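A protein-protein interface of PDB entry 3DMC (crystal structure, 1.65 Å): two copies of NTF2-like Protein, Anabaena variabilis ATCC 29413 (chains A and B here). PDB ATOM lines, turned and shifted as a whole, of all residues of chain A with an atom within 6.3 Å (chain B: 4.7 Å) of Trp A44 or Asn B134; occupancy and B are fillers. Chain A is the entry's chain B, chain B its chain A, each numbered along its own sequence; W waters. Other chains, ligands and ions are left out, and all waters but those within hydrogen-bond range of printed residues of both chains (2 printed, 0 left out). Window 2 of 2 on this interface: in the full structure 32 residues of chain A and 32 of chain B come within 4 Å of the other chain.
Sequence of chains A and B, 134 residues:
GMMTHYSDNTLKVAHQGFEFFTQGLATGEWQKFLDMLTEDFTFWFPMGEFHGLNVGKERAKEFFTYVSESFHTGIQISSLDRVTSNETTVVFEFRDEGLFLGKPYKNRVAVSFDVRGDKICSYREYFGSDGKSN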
ATOM      1  N   THR A  42      38.403 -21.707  10.660  1.00  0.00           N
ATOM      2  CA  THR A  42      37.095 -21.162  10.987  1.00  0.00           C
ATOM      3  C   THR A  42      36.836 -21.297  12.482  1.00  0.00           C
ATOM      4  O   THR A  42      37.374 -22.173  13.160  1.00  0.00           O
ATOM      5  CB  THR A  42      35.942 -21.843  10.236  1.00  0.00           C
ATOM      6  OG1 THR A  42      35.788 -23.206  10.689  1.00  0.00           O
ATOM      7  CG2 THR A  42      36.179 -21.823   8.704  1.00  0.00           C
ATOM      8  N   PHE A  43      36.019 -20.400  12.988  1.00  0.00           N
ATOM      9  CA  PHE A  43      35.582 -20.533  14.389  1.00  0.00           C
ATOM     10  C   PHE A  43      34.137 -20.162  14.582  1.00  0.00           C
ATOM     11  O   PHE A  43      33.581 -19.332  13.880  1.00  0.00           O
ATOM     12  CB  PHE A  43      36.477 -19.788  15.352  1.00  0.00           C
ATOM     13  CG  PHE A  43      36.508 -18.307  15.164  1.00  0.00           C
ATOM     14  CD1 PHE A  43      37.238 -17.743  14.119  1.00  0.00           C
ATOM     15  CD2 PHE A  43      35.870 -17.475  16.047  1.00  0.00           C
ATOM     16  CE1 PHE A  43      37.299 -16.378  13.970  1.00  0.00           C
ATOM     17  CE2 PHE A  43      35.925 -16.108  15.891  1.00  0.00           C
ATOM     18  CZ  PHE A  43      36.651 -15.561  14.843  1.00  0.00           C
ATOM     19  N   TRP A  44      33.534 -20.869  15.519  1.00  0.00           N
ATOM     20  CA  TRP A  44      32.130 -20.689  15.845  1.00  0.00           C
ATOM     21  C   TRP A  44      32.056 -20.245  17.311  1.00  0.00           C
ATOM     22  O   TRP A  44      32.700 -20.838  18.185  1.00  0.00           O
ATOM     23  CB  TRP A  44      31.369 -22.007  15.671  1.00  0.00           C
ATOM     24  CG  TRP A  44      30.173 -21.965  14.803  1.00  0.00           C
ATOM     25  CD1 TRP A  44      30.093 -22.393  13.520  1.00  0.00           C
ATOM     26  CD2 TRP A  44      28.858 -21.494  15.150  1.00  0.00           C
ATOM     27  NE1 TRP A  44      28.820 -22.205  13.032  1.00  0.00           N
ATOM     28  CE2 TRP A  44      28.043 -21.651  14.012  1.00  0.00           C
ATOM     29  CE3 TRP A  44      28.299 -20.926  16.302  1.00  0.00           C
ATOM     30  CZ2 TRP A  44      26.680 -21.274  13.996  1.00  0.00           C
ATOM     31  CZ3 TRP A  44      26.956 -20.574  16.293  1.00  0.00           C
ATOM     32  CH2 TRP A  44      26.162 -20.740  15.135  1.00  0.00           C
ATOM     33  N   PHE A  45      31.254 -19.212  17.539  1.00  0.00           N
ATOM     34  CA  PHE A  45      31.103 -18.570  18.842  1.00  0.00           C
ATOM     35  C   PHE A  45      29.620 -18.261  19.118  1.00  0.00           C
ATOM     36  O   PHE A  45      28.883 -17.996  18.215  1.00  0.00           O
ATOM     37  CB  PHE A  45      31.989 -17.292  18.916  1.00  0.00           C
ATOM     38  CG  PHE A  45      32.072 -16.680  20.308  1.00  0.00           C
ATOM     39  CD1 PHE A  45      32.945 -17.190  21.273  1.00  0.00           C
ATOM     40  CD2 PHE A  45      31.280 -15.588  20.650  1.00  0.00           C
ATOM     41  CE1 PHE A  45      33.018 -16.615  22.572  1.00  0.00           C
ATOM     42  CE2 PHE A  45      31.341 -15.035  21.924  1.00  0.00           C
ATOM     43  CZ  PHE A  45      32.213 -15.566  22.880  1.00  0.00           C
ATOM     44  N   PRO A  46      29.159 -18.350  20.384  1.00  0.00           N
ATOM     45  CA  PRO A  46      27.731 -18.348  20.590  1.00  0.00           C
ATOM     46  C   PRO A  46      26.980 -17.081  20.398  1.00  0.00           C
ATOM     47  O   PRO A  46      25.831 -17.142  20.040  1.00  0.00           O
ATOM     48  CB  PRO A  46      27.577 -18.797  22.049  1.00  0.00           C
ATOM     49  CG  PRO A  46      28.812 -19.537  22.373  1.00  0.00           C
ATOM     50  CD  PRO A  46      29.883 -18.878  21.549  1.00  0.00           C
ATOM     51  N   PHE A  50      30.729 -11.714  17.255  1.00  0.00           N
ATOM     52  CA  PHE A  50      31.363 -12.924  16.718  1.00  0.00           C
ATOM     53  C   PHE A  50      30.435 -14.142  16.716  1.00  0.00           C
ATOM     54  O   PHE A  50      30.858 -15.283  16.526  1.00  0.00           O
ATOM     55  CB  PHE A  50      32.704 -13.223  17.427  1.00  0.00           C
ATOM     56  CG  PHE A  50      33.753 -12.158  17.198  1.00  0.00           C
ATOM     57  CD1 PHE A  50      34.508 -12.171  16.047  1.00  0.00           C
ATOM     58  CD2 PHE A  50      33.923 -11.111  18.086  1.00  0.00           C
ATOM     59  CE1 PHE A  50      35.439 -11.183  15.791  1.00  0.00           C
ATOM     60  CE2 PHE A  50      34.877 -10.104  17.841  1.00  0.00           C
ATOM     61  CZ  PHE A  50      35.631 -10.158  16.686  1.00  0.00           C
ATOM     62  N   HIS A  51      29.149 -13.903  16.914  1.00  0.00           N
ATOM     63  CA  HIS A  51      28.195 -15.014  16.814  1.00  0.00           C
ATOM     64  C   HIS A  51      28.314 -15.749  15.500  1.00  0.00           C
ATOM     65  O   HIS A  51      28.461 -15.152  14.431  1.00  0.00           O
ATOM     66  CB  HIS A  51      26.749 -14.530  16.903  1.00  0.00           C
ATOM     67  CG  HIS A  51      25.762 -15.559  16.446  1.00  0.00           C
ATOM     68  ND1 HIS A  51      25.309 -16.566  17.273  1.00  0.00           N
ATOM     69  CD2 HIS A  51      25.167 -15.760  15.245  1.00  0.00           C
ATOM     70  CE1 HIS A  51      24.470 -17.336  16.605  1.00  0.00           C
ATOM     71  NE2 HIS A  51      24.368 -16.873  15.370  1.00  0.00           N
ATOM     72  N   GLY A  52      28.121 -17.051  15.590  1.00  0.00           N
ATOM     73  CA  GLY A  52      28.115 -17.955  14.452  1.00  0.00           C
ATOM     74  C   GLY A  52      29.466 -18.274  13.871  1.00  0.00           C
ATOM     75  O   GLY A  52      30.489 -18.304  14.569  1.00  0.00           O
ATOM     76  N   LEU A  53      29.449 -18.486  12.556  1.00  0.00           N
ATOM     77  CA  LEU A  53      30.641 -18.916  11.812  1.00  0.00           C
ATOM     78  C   LEU A  53      31.469 -17.721  11.389  1.00  0.00           C
ATOM     79  O   LEU A  53      30.972 -16.744  10.815  1.00  0.00           O
ATOM     80  CB  LEU A  53      30.282 -19.774  10.588  1.00  0.00           C
ATOM     81  CG  LEU A  53      31.500 -20.196   9.740  1.00  0.00           C
ATOM     82  CD1 LEU A  53      32.191 -21.395  10.367  1.00  0.00           C
ATOM     83  CD2 LEU A  53      31.087 -20.458   8.290  1.00  0.00           C
ATOM     84  N   ASN A  54      32.745 -17.820  11.724  1.00  0.00           N
ATOM     85  CA  ASN A  54      33.743 -16.820  11.385  1.00  0.00           C
ATOM     86  C   ASN A  54      34.840 -17.445  10.556  1.00  0.00           C
ATOM     87  O   ASN A  54      35.293 -18.520  10.860  1.00  0.00           O
ATOM     88  CB  ASN A  54      34.354 -16.266  12.661  1.00  0.00           C
ATOM     89  CG  ASN A  54      33.340 -15.595  13.558  1.00  0.00           C
ATOM     90  OD1 ASN A  54      33.143 -14.379  13.486  1.00  0.00           O
ATOM     91  ND2 ASN A  54      32.709 -16.384  14.449  1.00  0.00           N
ATOM     92  N   TYR A 123      37.640 -24.206  15.230  1.00  0.00           N
ATOM     93  CA  TYR A 123      37.403 -23.992  16.663  1.00  0.00           C
ATOM     94  C   TYR A 123      35.922 -23.763  16.885  1.00  0.00           C
ATOM     95  O   TYR A 123      35.290 -23.044  16.127  1.00  0.00           O
ATOM     96  CB  TYR A 123      38.209 -22.761  17.064  1.00  0.00           C
ATOM     97  CG  TYR A 123      38.003 -22.066  18.397  1.00  0.00           C
ATOM     98  CD1 TYR A 123      36.868 -21.290  18.682  1.00  0.00           C
ATOM     99  CD2 TYR A 123      39.007 -22.094  19.335  1.00  0.00           C
ATOM    100  CE1 TYR A 123      36.730 -20.603  19.932  1.00  0.00           C
ATOM    101  CE2 TYR A 123      38.892 -21.418  20.538  1.00  0.00           C
ATOM    102  CZ  TYR A 123      37.767 -20.659  20.829  1.00  0.00           C
ATOM    103  OH  TYR A 123      37.712 -20.015  22.044  1.00  0.00           O
ATOM    104  N   ARG A 124      35.410 -24.336  17.977  1.00  0.00           N
ATOM    105  CA  ARG A 124      34.046 -24.126  18.408  1.00  0.00           C
ATOM    106  C   ARG A 124      34.022 -23.971  19.922  1.00  0.00           C
ATOM    107  O   ARG A 124      34.608 -24.784  20.627  1.00  0.00           O
ATOM    108  CB  ARG A 124      33.163 -25.313  18.025  1.00  0.00           C
ATOM    109  CG  ARG A 124      32.962 -25.504  16.484  1.00  0.00           C
ATOM    110  CD  ARG A 124      32.523 -26.933  16.192  1.00  0.00           C
ATOM    111  NE  ARG A 124      33.576 -27.869  16.555  1.00  0.00           N
ATOM    112  CZ  ARG A 124      34.646 -28.113  15.824  1.00  0.00           C
ATOM    113  NH1 ARG A 124      34.797 -27.498  14.635  1.00  0.00           N
ATOM    114  NH2 ARG A 124      35.570 -28.937  16.278  1.00  0.00           N
ATOM    115  N   GLU A 125      33.390 -22.903  20.375  1.00  0.00           N
ATOM    116  CA  GLU A 125      33.240 -22.630  21.810  1.00  0.00           C
ATOM    117  C   GLU A 125      31.809 -22.758  22.269  1.00  0.00           C
ATOM    118  O   GLU A 125      30.860 -22.330  21.603  1.00  0.00           O
ATOM    119  CB  GLU A 125      33.770 -21.237  22.172  1.00  0.00           C
ATOM    120  CG  GLU A 125      33.689 -20.977  23.642  1.00  0.00           C
ATOM    121  CD  GLU A 125      34.388 -19.722  24.094  1.00  0.00           C
ATOM    122  OE1 GLU A 125      35.283 -19.217  23.386  1.00  0.00           O
ATOM    123  OE2 GLU A 125      34.017 -19.254  25.182  1.00  0.00           O
ATOM    124  N   TYR A 126      31.686 -23.378  23.437  1.00  0.00           N
ATOM    125  CA  TYR A 126      30.382 -23.573  24.092  1.00  0.00           C
ATOM    126  C   TYR A 126      30.456 -23.100  25.558  1.00  0.00           C
ATOM    127  O   TYR A 126      31.475 -23.299  26.225  1.00  0.00           O
ATOM    128  CB  TYR A 126      30.010 -25.057  24.074  1.00  0.00           C
ATOM    129  CG  TYR A 126      29.988 -25.767  22.739  1.00  0.00           C
ATOM    130  CD1 TYR A 126      31.167 -26.250  22.158  1.00  0.00           C
ATOM    131  CD2 TYR A 126      28.782 -25.975  22.041  1.00  0.00           C
ATOM    132  CE1 TYR A 126      31.139 -26.964  20.923  1.00  0.00           C
ATOM    133  CE2 TYR A 126      28.755 -26.643  20.786  1.00  0.00           C
ATOM    134  CZ  TYR A 126      29.953 -27.117  20.234  1.00  0.00           C
ATOM    135  OH  TYR A 126      29.887 -27.771  19.031  1.00  0.00           O
ATOM    136  N   SER B  78      19.067 -32.186  14.434  1.00  0.00           N
ATOM    137  CA  SER B  78      19.188 -31.863  13.014  1.00  0.00           C
ATOM    138  C   SER B  78      20.442 -32.521  12.446  1.00  0.00           C
ATOM    139  O   SER B  78      20.471 -33.040  11.334  1.00  0.00           O
ATOM    140  CB  SER B  78      19.216 -30.335  12.801  1.00  0.00           C
ATOM    141  OG  SER B  78      18.018 -29.721  13.289  1.00  0.00           O
ATOM    142  N   ARG B  95      23.429 -30.172  16.566  1.00  0.00           N
ATOM    143  CA  ARG B  95      22.552 -29.033  16.205  1.00  0.00           C
ATOM    144  C   ARG B  95      21.132 -29.505  16.391  1.00  0.00           C
ATOM    145  O   ARG B  95      20.812 -30.656  16.037  1.00  0.00           O
ATOM    146  CB  ARG B  95      22.795 -28.569  14.741  1.00  0.00           C
ATOM    147  CG  ARG B  95      24.177 -27.950  14.477  1.00  0.00           C
ATOM    148  CD  ARG B  95      24.568 -27.863  13.007  1.00  0.00           C
ATOM    149  NE  ARG B  95      23.531 -27.110  12.277  1.00  0.00           N
ATOM    150  CZ  ARG B  95      22.583 -27.673  11.519  1.00  0.00           C
ATOM    151  NH1 ARG B  95      22.537 -28.992  11.365  1.00  0.00           N
ATOM    152  NH2 ARG B  95      21.670 -26.910  10.908  1.00  0.00           N
ATOM    153  N   ASP B  96      20.302 -28.662  17.016  1.00  0.00           N
ATOM    154  CA  ASP B  96      18.937 -29.050  17.289  1.00  0.00           C
ATOM    155  C   ASP B  96      17.947 -27.941  16.978  1.00  0.00           C
ATOM    156  O   ASP B  96      18.300 -26.765  16.729  1.00  0.00           O
ATOM    157  CB  ASP B  96      18.771 -29.651  18.696  1.00  0.00           C
ATOM    158  CG  ASP B  96      18.971 -28.655  19.838  1.00  0.00           C
ATOM    159  OD1 ASP B  96      19.258 -27.463  19.589  1.00  0.00           O
ATOM    160  OD2 ASP B  96      18.838 -29.121  21.007  1.00  0.00           O
ATOM    161  N   LYS B 106      16.363 -22.883  17.823  1.00  0.00           N
ATOM    162  CA  LYS B 106      17.458 -23.588  17.165  1.00  0.00           C
ATOM    163  C   LYS B 106      18.724 -23.364  17.950  1.00  0.00           C
ATOM    164  O   LYS B 106      18.951 -22.268  18.444  1.00  0.00           O
ATOM    165  CB  LYS B 106      17.669 -23.060  15.759  1.00  0.00           C
ATOM    166  CG  LYS B 106      16.512 -23.276  14.822  1.00  0.00           C
ATOM    167  CD  LYS B 106      16.792 -22.610  13.492  1.00  0.00           C
ATOM    168  CE  LYS B 106      17.690 -23.478  12.618  1.00  0.00           C
ATOM    169  NZ  LYS B 106      17.628 -23.102  11.164  1.00  0.00           N
ATOM    170  N   ASN B 107      19.536 -24.400  18.095  1.00  0.00           N
ATOM    171  CA  ASN B 107      20.795 -24.250  18.830  1.00  0.00           C
ATOM    172  C   ASN B 107      21.911 -25.191  18.404  1.00  0.00           C
ATOM    173  O   ASN B 107      21.734 -26.143  17.626  1.00  0.00           O
ATOM    174  CB  ASN B 107      20.528 -24.381  20.333  1.00  0.00           C
ATOM    175  CG  ASN B 107      21.291 -23.376  21.168  1.00  0.00           C
ATOM    176  OD1 ASN B 107      22.187 -22.661  20.685  1.00  0.00           O
ATOM    177  ND2 ASN B 107      20.945 -23.322  22.475  1.00  0.00           N
ATOM    178  N   ARG B 108      23.079 -24.862  18.906  1.00  0.00           N
ATOM    179  CA  ARG B 108      24.228 -25.723  18.895  1.00  0.00           C
ATOM    180  C   ARG B 108      24.463 -26.088  20.351  1.00  0.00           C
ATOM    181  O   ARG B 108      24.312 -25.254  21.251  1.00  0.00           O
ATOM    182  CB  ARG B 108      25.475 -25.061  18.284  1.00  0.00           C
ATOM    183  CG  ARG B 108      25.426 -24.888  16.769  1.00  0.00           C
ATOM    184  CD  ARG B 108      26.711 -24.430  16.176  1.00  0.00           C
ATOM    185  NE  ARG B 108      26.700 -24.689  14.732  1.00  0.00           N
ATOM    186  CZ  ARG B 108      27.752 -25.108  14.041  1.00  0.00           C
ATOM    187  NH1 ARG B 108      28.914 -25.336  14.643  1.00  0.00           N
ATOM    188  NH2 ARG B 108      27.643 -25.291  12.739  1.00  0.00           N
ATOM    189  N   GLY B 128      26.149 -23.552  22.417  1.00  0.00           N
ATOM    190  CA  GLY B 128      27.060 -23.114  21.357  1.00  0.00           C
ATOM    191  C   GLY B 128      26.520 -22.046  20.433  1.00  0.00           C
ATOM    192  O   GLY B 128      27.239 -21.557  19.580  1.00  0.00           O
ATOM    193  N   SER B 129      25.236 -21.718  20.578  1.00  0.00           N
ATOM    194  CA  SER B 129      24.634 -20.618  19.837  1.00  0.00           C
ATOM    195  C   SER B 129      23.672 -19.824  20.731  1.00  0.00           C
ATOM    196  O   SER B 129      23.719 -19.904  21.970  1.00  0.00           O
ATOM    197  CB  SER B 129      23.940 -21.143  18.574  1.00  0.00           C
ATOM    198  OG  SER B 129      23.605 -20.116  17.631  1.00  0.00           O
ATOM    199  N   SER B 133      19.484 -19.835  16.081  1.00  0.00           N
ATOM    200  CA  SER B 133      20.303 -20.184  14.933  1.00  0.00           C
ATOM    201  C   SER B 133      21.278 -21.294  15.278  1.00  0.00           C
ATOM    202  O   SER B 133      21.622 -21.504  16.453  1.00  0.00           O
ATOM    203  CB  SER B 133      21.121 -18.978  14.490  1.00  0.00           C
ATOM    204  OG  SER B 133      22.090 -18.638  15.480  1.00  0.00           O
ATOM    205  N   ASN B 134      21.711 -22.005  14.252  1.00  0.00           N
ATOM    206  CA  ASN B 134      22.707 -23.050  14.452  1.00  0.00           C
ATOM    207  C   ASN B 134      23.540 -23.363  13.201  1.00  0.00           C
ATOM    208  O   ASN B 134      24.210 -24.413  13.094  1.00  0.00           O
ATOM    209  CB  ASN B 134      22.006 -24.296  14.968  1.00  0.00           C
ATOM    210  CG  ASN B 134      21.039 -24.878  13.957  1.00  0.00           C
ATOM    211  OD1 ASN B 134      21.110 -24.550  12.769  1.00  0.00           O
ATOM    212  ND2 ASN B 134      20.149 -25.765  14.411  1.00  0.00           N
ATOM    213  OXT ASN B 134      23.560 -22.529  12.273  1.00  0.00           O
HETATM  214  O   HOH W   1      29.743 -25.032  17.479  1.00  0.00           O
HETATM  215  O   HOH W   2      29.678 -22.827  19.050  1.00  0.00           O
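Of chain B, only Arg B108, Gly B128, Ser B129 and Asn B134 come within 4 Å of Trp A44.
Asn B134 touches just one residue of chain A: Trp A44.
Printed residues of chain A within 4 Å of Ser B133: His A51 (2.9 Å).
Of the printed residues of chain A, Ser B129 touches Trp A44, Pro A46 and His A51.
Of the printed residues of chain B, Tyr A126 touches Gly B128 (3.4 Å).
Of the printed residues of chain B, Pro A46 touches Gly B128 (3.4 Å) and Ser B129 (3.5 Å).
Of the printed residues of chain B, Glu A125 touches Gly B128 (3.9 Å).
The nearest residue of chain A that does not touch Asn B134 is His A51 (5.9 Å).
The side-chain hydroxyl (OH) of Tyr A123 lies within hydrogen-bond range of the side-chain carboxylate (OE1) of Glu A125 (2.9 Å).
The backbone carbonyl oxygen (O) of Asp B96 sits at hydrogen-bond distance from the side-chain amide nitrogen (ND2) of Asn B134 (3.1 Å).
NE of Arg B108 lies within salt-bridge range of O of Asn B134, at 3.0 Å.
The backbone carbonyl oxygen (O) of Trp A44 sits at hydrogen-bond distance from the backbone NH (N) of Glu A125, 3.1 Å away.
The backbone carbonyl oxygen (O) of Lys B106 lies within hydrogen-bond range of the backbone NH (N) of Ser B133 (3.4 Å).
A ring nitrogen (ND1) of His A51 lies within hydrogen-bond range of the backbone carbonyl oxygen (O) of Pro A46, 2.9 Å away.
No position is printed for both chains.
Of the 14 printed residues of chain A, 5 touch a printed residue of chain B.
Hydrophobic or aromatic side chains of chain A that line the printed part of chain B: Trp A44, Pro A46, His A51 and Tyr A126.
Among the printed residues, 10 pairs touch across the chains.
Among the printed residues, no Asp or Glu carboxylate lies within 4 Å of a Lys or Arg side-chain nitrogen of the other chain.
Among the printed residues, merely in contact across the chains: His A51 with Ser B129 (3.1 Å), Pro A46 with Gly B128 (3.4 Å), Tyr A126 with Gly B128 (3.4 Å), Trp A44 with Gly B128 (3.4 Å), Pro A46 with Ser B129 (3.5 Å), Trp A44 with Ser B129 (3.6 Å), Trp A44 with Asn B134 (3.8 Å) and Glu A125 with Gly B128 (3.9 Å).
Water W2 bridges O of Gly B128 (2.8 Å) and O of Glu A125 (2.9 Å).
Water W1 bridges the guanidinium group (NH1) of Arg B108 (3.0 Å) and the side-chain hydroxyl (OH) of Tyr A126 (3.2 Å).
NH2 of Arg B108 lies close to NE1 of Trp A44, at 3.3 Å.
NE2 of His A51 sits at hydrogen-bond distance from OG of Ser B133 (2.9 Å).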
